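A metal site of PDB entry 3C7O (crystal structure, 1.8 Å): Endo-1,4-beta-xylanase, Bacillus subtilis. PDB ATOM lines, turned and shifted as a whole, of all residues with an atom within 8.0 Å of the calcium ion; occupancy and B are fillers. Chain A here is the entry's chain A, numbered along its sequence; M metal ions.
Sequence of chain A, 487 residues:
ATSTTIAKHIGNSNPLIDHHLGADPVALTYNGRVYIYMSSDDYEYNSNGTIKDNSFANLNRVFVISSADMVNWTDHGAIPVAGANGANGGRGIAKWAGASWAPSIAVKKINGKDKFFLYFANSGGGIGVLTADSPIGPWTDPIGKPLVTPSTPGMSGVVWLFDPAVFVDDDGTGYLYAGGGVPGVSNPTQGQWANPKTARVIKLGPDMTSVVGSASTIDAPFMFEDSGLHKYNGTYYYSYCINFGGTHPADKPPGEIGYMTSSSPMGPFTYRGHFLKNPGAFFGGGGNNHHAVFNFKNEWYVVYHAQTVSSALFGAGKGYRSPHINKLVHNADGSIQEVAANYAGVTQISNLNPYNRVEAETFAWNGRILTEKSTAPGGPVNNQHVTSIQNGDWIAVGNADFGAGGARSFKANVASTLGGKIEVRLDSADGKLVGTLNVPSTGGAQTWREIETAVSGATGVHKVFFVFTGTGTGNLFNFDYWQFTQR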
ATOM      1  N   THR A  74     -16.832 -22.793   7.471  1.00  0.00           N
ATOM      2  CA  THR A  74     -17.238 -21.527   8.045  1.00  0.00           C
ATOM      3  C   THR A  74     -15.988 -20.689   8.240  1.00  0.00           C
ATOM      4  O   THR A  74     -15.016 -21.153   8.853  1.00  0.00           O
ATOM      5  CB  THR A  74     -17.906 -21.732   9.429  1.00  0.00           C
ATOM      6  OG1 THR A  74     -19.011 -22.635   9.305  1.00  0.00           O
ATOM      7  CG2 THR A  74     -18.399 -20.407   9.989  1.00  0.00           C
ATOM      8  N   ASP A  75     -15.998 -19.489   7.677  1.00  0.00           N
ATOM      9  CA  ASP A  75     -14.913 -18.565   7.883  1.00  0.00           C
ATOM     10  C   ASP A  75     -15.118 -17.766   9.181  1.00  0.00           C
ATOM     11  O   ASP A  75     -16.086 -17.039   9.301  1.00  0.00           O
ATOM     12  CB  ASP A  75     -14.720 -17.632   6.690  1.00  0.00           C
ATOM     13  CG  ASP A  75     -13.303 -17.109   6.613  1.00  0.00           C
ATOM     14  OD1 ASP A  75     -12.796 -16.652   7.660  1.00  0.00           O
ATOM     15  OD2 ASP A  75     -12.695 -17.204   5.532  1.00  0.00           O
ATOM     16  N   ARG A 357     -29.872 -21.504  11.328  1.00  0.00           N
ATOM     17  CA  ARG A 357     -29.141 -20.364  10.820  1.00  0.00           C
ATOM     18  C   ARG A 357     -27.797 -20.900  10.320  1.00  0.00           C
ATOM     19  O   ARG A 357     -27.099 -21.627  11.048  1.00  0.00           O
ATOM     20  CB  ARG A 357     -28.939 -19.277  11.898  1.00  0.00           C
ATOM     21  CG  ARG A 357     -27.906 -18.232  11.481  1.00  0.00           C
ATOM     22  CD  ARG A 357     -27.635 -17.159  12.549  1.00  0.00           C
ATOM     23  NE  ARG A 357     -26.445 -16.379  12.231  1.00  0.00           N
ATOM     24  CZ  ARG A 357     -26.223 -15.120  12.625  1.00  0.00           C
ATOM     25  NH1 ARG A 357     -27.145 -14.464  13.339  1.00  0.00           N
ATOM     26  NH2 ARG A 357     -25.096 -14.505  12.296  1.00  0.00           N
ATOM     27  N   VAL A 358     -27.470 -20.578   9.062  1.00  0.00           N
ATOM     28  CA  VAL A 358     -26.190 -20.953   8.455  1.00  0.00           C
ATOM     29  C   VAL A 358     -25.539 -19.636   8.039  1.00  0.00           C
ATOM     30  O   VAL A 358     -26.156 -18.813   7.385  1.00  0.00           O
ATOM     31  CB  VAL A 358     -26.354 -21.895   7.238  1.00  0.00           C
ATOM     32  CG1 VAL A 358     -24.967 -22.240   6.601  1.00  0.00           C
ATOM     33  CG2 VAL A 358     -27.090 -23.176   7.634  1.00  0.00           C
ATOM     34  N   GLU A 359     -24.291 -19.437   8.465  1.00  0.00           N
ATOM     35  CA  GLU A 359     -23.589 -18.218   8.100  1.00  0.00           C
ATOM     36  C   GLU A 359     -23.412 -18.165   6.577  1.00  0.00           C
ATOM     37  O   GLU A 359     -23.125 -19.191   5.944  1.00  0.00           O
ATOM     38  CB  GLU A 359     -22.227 -18.199   8.779  1.00  0.00           C
ATOM     39  CG  GLU A 359     -22.274 -18.141  10.316  1.00  0.00           C
ATOM     40  CD  GLU A 359     -23.229 -17.080  10.832  1.00  0.00           C
ATOM     41  OE1 GLU A 359     -23.262 -15.936  10.297  1.00  0.00           O
ATOM     42  OE2 GLU A 359     -23.952 -17.401  11.796  1.00  0.00           O
ATOM     43  N   ALA A 360     -23.542 -16.982   5.992  1.00  0.00           N
ATOM     44  CA  ALA A 360     -23.259 -16.805   4.562  1.00  0.00           C
ATOM     45  C   ALA A 360     -21.813 -17.194   4.269  1.00  0.00           C
ATOM     46  O   ALA A 360     -21.518 -17.707   3.189  1.00  0.00           O
ATOM     47  CB  ALA A 360     -23.529 -15.373   4.145  1.00  0.00           C
ATOM     48  N   GLU A 361     -20.926 -16.931   5.234  1.00  0.00           N
ATOM     49  CA  GLU A 361     -19.499 -17.307   5.153  1.00  0.00           C
ATOM     50  C   GLU A 361     -19.232 -18.798   5.462  1.00  0.00           C
ATOM     51  O   GLU A 361     -18.082 -19.215   5.644  1.00  0.00           O
ATOM     52  CB  GLU A 361     -18.669 -16.406   6.073  1.00  0.00           C
ATOM     53  CG  GLU A 361     -18.932 -16.609   7.583  1.00  0.00           C
ATOM     54  CD  GLU A 361     -20.040 -15.712   8.142  1.00  0.00           C
ATOM     55  OE1 GLU A 361     -20.926 -15.227   7.382  1.00  0.00           O
ATOM     56  OE2 GLU A 361     -20.035 -15.498   9.375  1.00  0.00           O
ATOM     57  N   THR A 362     -20.295 -19.601   5.507  1.00  0.00           N
ATOM     58  CA  THR A 362     -20.177 -21.071   5.552  1.00  0.00           C
ATOM     59  C   THR A 362     -20.506 -21.563   4.139  1.00  0.00           C
ATOM     60  O   THR A 362     -21.661 -21.527   3.716  1.00  0.00           O
ATOM     61  CB  THR A 362     -21.167 -21.695   6.558  1.00  0.00           C
ATOM     62  OG1 THR A 362     -20.827 -21.250   7.875  1.00  0.00           O
ATOM     63  CG2 THR A 362     -21.126 -23.223   6.484  1.00  0.00           C
ATOM     64  N   GLU A 372     -15.196 -10.831   5.350  1.00  0.00           N
ATOM     65  CA  GLU A 372     -14.630  -9.891   6.308  1.00  0.00           C
ATOM     66  C   GLU A 372     -15.525  -9.803   7.532  1.00  0.00           C
ATOM     67  O   GLU A 372     -16.662 -10.242   7.540  1.00  0.00           O
ATOM     68  CB  GLU A 372     -14.482  -8.507   5.671  1.00  0.00           C
ATOM     69  CG  GLU A 372     -15.805  -7.880   5.360  1.00  0.00           C
ATOM     70  CD  GLU A 372     -15.707  -6.500   4.792  1.00  0.00           C
ATOM     71  OE1 GLU A 372     -14.580  -6.019   4.532  1.00  0.00           O
ATOM     72  OE2 GLU A 372     -16.778  -5.896   4.598  1.00  0.00           O
ATOM     73  N   SER A 374     -17.994  -8.287  10.362  1.00  0.00           N
ATOM     74  CA  SER A 374     -19.308  -8.039   9.747  1.00  0.00           C
ATOM     75  C   SER A 374     -19.779  -7.005  10.799  1.00  0.00           C
ATOM     76  O   SER A 374     -19.490  -7.164  12.004  1.00  0.00           O
ATOM     77  CB  SER A 374     -20.306  -9.163   9.757  1.00  0.00           C
ATOM     78  OG  SER A 374     -21.545  -8.590   9.343  1.00  0.00           O
ATOM     79  N   ALA A 376     -22.975  -6.622  11.261  1.00  0.00           N
ATOM     80  CA  ALA A 376     -24.327  -7.121  11.548  1.00  0.00           C
ATOM     81  C   ALA A 376     -24.545  -7.295  13.037  1.00  0.00           C
ATOM     82  O   ALA A 376     -23.678  -7.819  13.726  1.00  0.00           O
ATOM     83  CB  ALA A 376     -24.586  -8.442  10.831  1.00  0.00           C
ATOM     84  N   GLY A 378     -25.559  -8.991  16.418  1.00  0.00           N
ATOM     85  CA  GLY A 378     -25.641 -10.359  16.889  1.00  0.00           C
ATOM     86  C   GLY A 378     -24.671 -11.271  16.156  1.00  0.00           C
ATOM     87  O   GLY A 378     -23.628 -10.817  15.696  1.00  0.00           O
ATOM     88  N   GLY A 379     -25.022 -12.547  16.048  1.00  0.00           N
ATOM     89  CA  GLY A 379     -24.148 -13.507  15.380  1.00  0.00           C
ATOM     90  C   GLY A 379     -23.076 -14.091  16.272  1.00  0.00           C
ATOM     91  O   GLY A 379     -22.957 -13.707  17.447  1.00  0.00           O
ATOM     92  N   PRO A 380     -22.289 -15.051  15.725  1.00  0.00           N
ATOM     93  CA  PRO A 380     -21.273 -15.736  16.510  1.00  0.00           C
ATOM     94  C   PRO A 380     -20.062 -14.843  16.796  1.00  0.00           C
ATOM     95  O   PRO A 380     -19.955 -13.733  16.248  1.00  0.00           O
ATOM     96  CB  PRO A 380     -20.888 -16.933  15.627  1.00  0.00           C
ATOM     97  CG  PRO A 380     -21.201 -16.510  14.228  1.00  0.00           C
ATOM     98  CD  PRO A 380     -22.356 -15.540  14.334  1.00  0.00           C
ATOM     99  N   ASN A 382     -16.715 -13.082  16.443  1.00  0.00           N
ATOM    100  CA  ASN A 382     -16.007 -12.646  15.240  1.00  0.00           C
ATOM    101  C   ASN A 382     -16.810 -12.872  13.977  1.00  0.00           C
ATOM    102  O   ASN A 382     -16.244 -13.133  12.926  1.00  0.00           O
ATOM    103  CB  ASN A 382     -14.627 -13.309  15.120  1.00  0.00           C
ATOM    104  CG  ASN A 382     -13.589 -12.374  14.513  1.00  0.00           C
ATOM    105  OD1 ASN A 382     -13.609 -11.171  14.753  1.00  0.00           O
ATOM    106  ND2 ASN A 382     -12.666 -12.934  13.730  1.00  0.00           N
ATOM    107  N   ASN A 383     -18.125 -12.736  14.092  1.00  0.00           N
ATOM    108  CA  ASN A 383     -19.028 -12.930  12.954  1.00  0.00           C
ATOM    109  C   ASN A 383     -18.540 -12.212  11.716  1.00  0.00           C
ATOM    110  O   ASN A 383     -18.167 -11.040  11.764  1.00  0.00           O
ATOM    111  CB  ASN A 383     -20.439 -12.439  13.312  1.00  0.00           C
ATOM    112  CG  ASN A 383     -21.428 -12.598  12.155  1.00  0.00           C
ATOM    113  OD1 ASN A 383     -21.460 -13.629  11.465  1.00  0.00           O
ATOM    114  ND2 ASN A 383     -22.274 -11.595  11.959  1.00  0.00           N
ATOM    115  N   GLN A 384     -18.574 -12.939  10.601  1.00  0.00           N
ATOM    116  CA  GLN A 384     -18.124 -12.404   9.325  1.00  0.00           C
ATOM    117  C   GLN A 384     -19.312 -12.187   8.392  1.00  0.00           C
ATOM    118  O   GLN A 384     -20.440 -12.556   8.719  1.00  0.00           O
ATOM    119  CB  GLN A 384     -17.144 -13.369   8.658  1.00  0.00           C
ATOM    120  CG  GLN A 384     -15.970 -13.757   9.545  1.00  0.00           C
ATOM    121  CD  GLN A 384     -14.884 -12.713   9.575  1.00  0.00           C
ATOM    122  OE1 GLN A 384     -14.257 -12.419   8.540  1.00  0.00           O
ATOM    123  NE2 GLN A 384     -14.616 -12.148  10.775  1.00  0.00           N
ATOM    124  N   HIS A 385     -19.050 -11.575   7.231  1.00  0.00           N
ATOM    125  CA  HIS A 385     -20.032 -11.595   6.155  1.00  0.00           C
ATOM    126  C   HIS A 385     -19.359 -11.821   4.803  1.00  0.00           C
ATOM    127  O   HIS A 385     -18.135 -11.719   4.694  1.00  0.00           O
ATOM    128  CB  HIS A 385     -20.972 -10.370   6.161  1.00  0.00           C
ATOM    129  CG  HIS A 385     -20.286  -9.050   5.961  1.00  0.00           C
ATOM    130  ND1 HIS A 385     -20.613  -7.926   6.701  1.00  0.00           N
ATOM    131  CD2 HIS A 385     -19.317  -8.659   5.102  1.00  0.00           C
ATOM    132  CE1 HIS A 385     -19.864  -6.911   6.312  1.00  0.00           C
ATOM    133  NE2 HIS A 385     -19.068  -7.328   5.339  1.00  0.00           N
ATOM    134  N   VAL A 386     -20.158 -12.189   3.807  1.00  0.00           N
ATOM    135  CA  VAL A 386     -19.687 -12.276   2.416  1.00  0.00           C
ATOM    136  C   VAL A 386     -19.795 -10.892   1.811  1.00  0.00           C
ATOM    137  O   VAL A 386     -20.836 -10.218   1.896  1.00  0.00           O
ATOM    138  CB  VAL A 386     -20.500 -13.331   1.595  1.00  0.00           C
ATOM    139  CG1 VAL A 386     -20.079 -13.354   0.103  1.00  0.00           C
ATOM    140  CG2 VAL A 386     -20.335 -14.714   2.235  1.00  0.00           C
ATOM    141  N   ASN A 413     -29.967 -12.367   5.831  1.00  0.00           N
ATOM    142  CA  ASN A 413     -29.615 -11.110   6.459  1.00  0.00           C
ATOM    143  C   ASN A 413     -28.625 -10.366   5.566  1.00  0.00           C
ATOM    144  O   ASN A 413     -27.527 -10.862   5.285  1.00  0.00           O
ATOM    145  CB  ASN A 413     -28.988 -11.376   7.835  1.00  0.00           C
ATOM    146  CG  ASN A 413     -29.067 -10.159   8.752  1.00  0.00           C
ATOM    147  OD1 ASN A 413     -30.064  -9.444   8.745  1.00  0.00           O
ATOM    148  ND2 ASN A 413     -28.013  -9.934   9.560  1.00  0.00           N
ATOM    149  N   TRP A 448     -28.685  -3.420   8.340  1.00  0.00           N
ATOM    150  CA  TRP A 448     -29.033  -4.813   8.106  1.00  0.00           C
ATOM    151  C   TRP A 448     -30.508  -5.091   8.146  1.00  0.00           C
ATOM    152  O   TRP A 448     -31.233  -4.568   9.001  1.00  0.00           O
ATOM    153  CB  TRP A 448     -28.283  -5.699   9.101  1.00  0.00           C
ATOM    154  CG  TRP A 448     -26.803  -5.594   8.879  1.00  0.00           C
ATOM    155  CD1 TRP A 448     -25.951  -4.683   9.437  1.00  0.00           C
ATOM    156  CD2 TRP A 448     -26.009  -6.394   7.990  1.00  0.00           C
ATOM    157  NE1 TRP A 448     -24.676  -4.865   8.956  1.00  0.00           N
ATOM    158  CE2 TRP A 448     -24.683  -5.901   8.057  1.00  0.00           C
ATOM    159  CE3 TRP A 448     -26.300  -7.459   7.119  1.00  0.00           C
ATOM    160  CZ2 TRP A 448     -23.625  -6.478   7.331  1.00  0.00           C
ATOM    161  CZ3 TRP A 448     -25.241  -8.023   6.388  1.00  0.00           C
ATOM    162  CH2 TRP A 448     -23.922  -7.520   6.507  1.00  0.00           C
ATOM    163  N   PHE A 479     -23.584  -9.904   3.010  1.00  0.00           N
ATOM    164  CA  PHE A 479     -24.458 -11.030   3.231  1.00  0.00           C
ATOM    165  C   PHE A 479     -24.061 -12.012   4.358  1.00  0.00           C
ATOM    166  O   PHE A 479     -22.916 -12.503   4.340  1.00  0.00           O
ATOM    167  CB  PHE A 479     -24.526 -11.790   1.880  1.00  0.00           C
ATOM    168  CG  PHE A 479     -25.354 -13.085   1.870  1.00  0.00           C
ATOM    169  CD1 PHE A 479     -26.444 -13.295   2.739  1.00  0.00           C
ATOM    170  CD2 PHE A 479     -25.092 -14.040   0.892  1.00  0.00           C
ATOM    171  CE1 PHE A 479     -27.197 -14.495   2.669  1.00  0.00           C
ATOM    172  CE2 PHE A 479     -25.841 -15.237   0.808  1.00  0.00           C
ATOM    173  CZ  PHE A 479     -26.908 -15.460   1.709  1.00  0.00           C
ATOM    174  N   ASP A 480     -24.838 -12.166   5.433  1.00  0.00           N
ATOM    175  CA  ASP A 480     -24.320 -12.158   6.811  1.00  0.00           C
ATOM    176  C   ASP A 480     -24.683 -13.640   7.153  1.00  0.00           C
ATOM    177  O   ASP A 480     -23.837 -14.431   7.554  1.00  0.00           O
ATOM    178  CB  ASP A 480     -25.015 -11.240   7.820  1.00  0.00           C
ATOM    179  CG  ASP A 480     -24.722 -11.672   9.280  1.00  0.00           C
ATOM    180  OD1 ASP A 480     -23.635 -12.261   9.583  1.00  0.00           O
ATOM    181  OD2 ASP A 480     -25.607 -11.450  10.127  1.00  0.00           O
ATOM    182  N   TYR A 481     -25.957 -14.002   6.969  1.00  0.00           N
ATOM    183  CA  TYR A 481     -26.427 -15.391   7.195  1.00  0.00           C
ATOM    184  C   TYR A 481     -27.707 -15.691   6.403  1.00  0.00           C
ATOM    185  O   TYR A 481     -28.355 -14.767   5.866  1.00  0.00           O
ATOM    186  CB  TYR A 481     -26.679 -15.695   8.695  1.00  0.00           C
ATOM    187  CG  TYR A 481     -27.892 -14.981   9.297  1.00  0.00           C
ATOM    188  CD1 TYR A 481     -29.183 -15.486   9.132  1.00  0.00           C
ATOM    189  CD2 TYR A 481     -27.717 -13.812  10.039  1.00  0.00           C
ATOM    190  CE1 TYR A 481     -30.297 -14.798   9.670  1.00  0.00           C
ATOM    191  CE2 TYR A 481     -28.809 -13.129  10.588  1.00  0.00           C
ATOM    192  CZ  TYR A 481     -30.095 -13.642  10.400  1.00  0.00           C
ATOM    193  OH  TYR A 481     -31.169 -12.969  10.943  1.00  0.00           O
ATOM    194  N   TRP A 482     -28.060 -16.961   6.355  1.00  0.00           N
ATOM    195  CA  TRP A 482     -29.318 -17.358   5.739  1.00  0.00           C
ATOM    196  C   TRP A 482     -29.953 -18.482   6.530  1.00  0.00           C
ATOM    197  O   TRP A 482     -29.309 -19.090   7.404  1.00  0.00           O
ATOM    198  CB  TRP A 482     -29.104 -17.737   4.269  1.00  0.00           C
ATOM    199  CG  TRP A 482     -27.997 -18.741   3.991  1.00  0.00           C
ATOM    200  CD1 TRP A 482     -26.708 -18.469   3.621  1.00  0.00           C
ATOM    201  CD2 TRP A 482     -28.110 -20.164   4.030  1.00  0.00           C
ATOM    202  NE1 TRP A 482     -25.994 -19.650   3.426  1.00  0.00           N
ATOM    203  CE2 TRP A 482     -26.835 -20.708   3.676  1.00  0.00           C
ATOM    204  CE3 TRP A 482     -29.155 -21.049   4.322  1.00  0.00           C
ATOM    205  CZ2 TRP A 482     -26.598 -22.088   3.602  1.00  0.00           C
ATOM    206  CZ3 TRP A 482     -28.916 -22.424   4.264  1.00  0.00           C
ATOM    207  CH2 TRP A 482     -27.654 -22.923   3.908  1.00  0.00           C
HETATM  208 CA    CA M   1     -22.093 -14.171   9.311  1.00  0.00          CA
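The backbone carbonyl oxygen of Asn 383 is in hydrogen-bond range of the backbone NH of Ser 374, 3.1 Å away. The side-chain carboxylate (OE2) of Glu 359 is in salt-bridge range of the guanidinium group (NE) of Arg 357, at 2.7 Å. OE1 of Gln 384 lies close to O of Glu 372 (3.4 Å). NE2 of Gln 384 is in hydrogen-bond range of O of Asn 382 (2.9 Å). The backbone carbonyl oxygen (O) of Glu 361 is in hydrogen-bond range of the backbone NH (N) of Asp 75. The guanidinium group (NH2) of Arg 357 is in salt-bridge range of the side-chain carboxylate (OD2) of Asp 480 (3.8 Å). O of Asp 480 sits close to N of Ala 360. The side-chain amide nitrogen of Asn 413 lies within hydrogen-bond range of the side-chain carboxylate of Asp 480, at 2.9 Å.
The calcium ion is bound by OD1 of Asn 383 (2.3 Å), OE1 of Glu 359 (2.3 Å), O of Gln 384 (2.4 Å), OE2 of Glu 361 (2.4 Å), OD1 of Asp 480 (2.5 Å), O of Asp 480 (2.5 Å) and OE1 of Glu 361 (2.5 Å).
Five residues have an atom within 4 Å of the calcium ion: Glu 359, Glu 361, Asn 383, Gln 384 and Asp 480.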
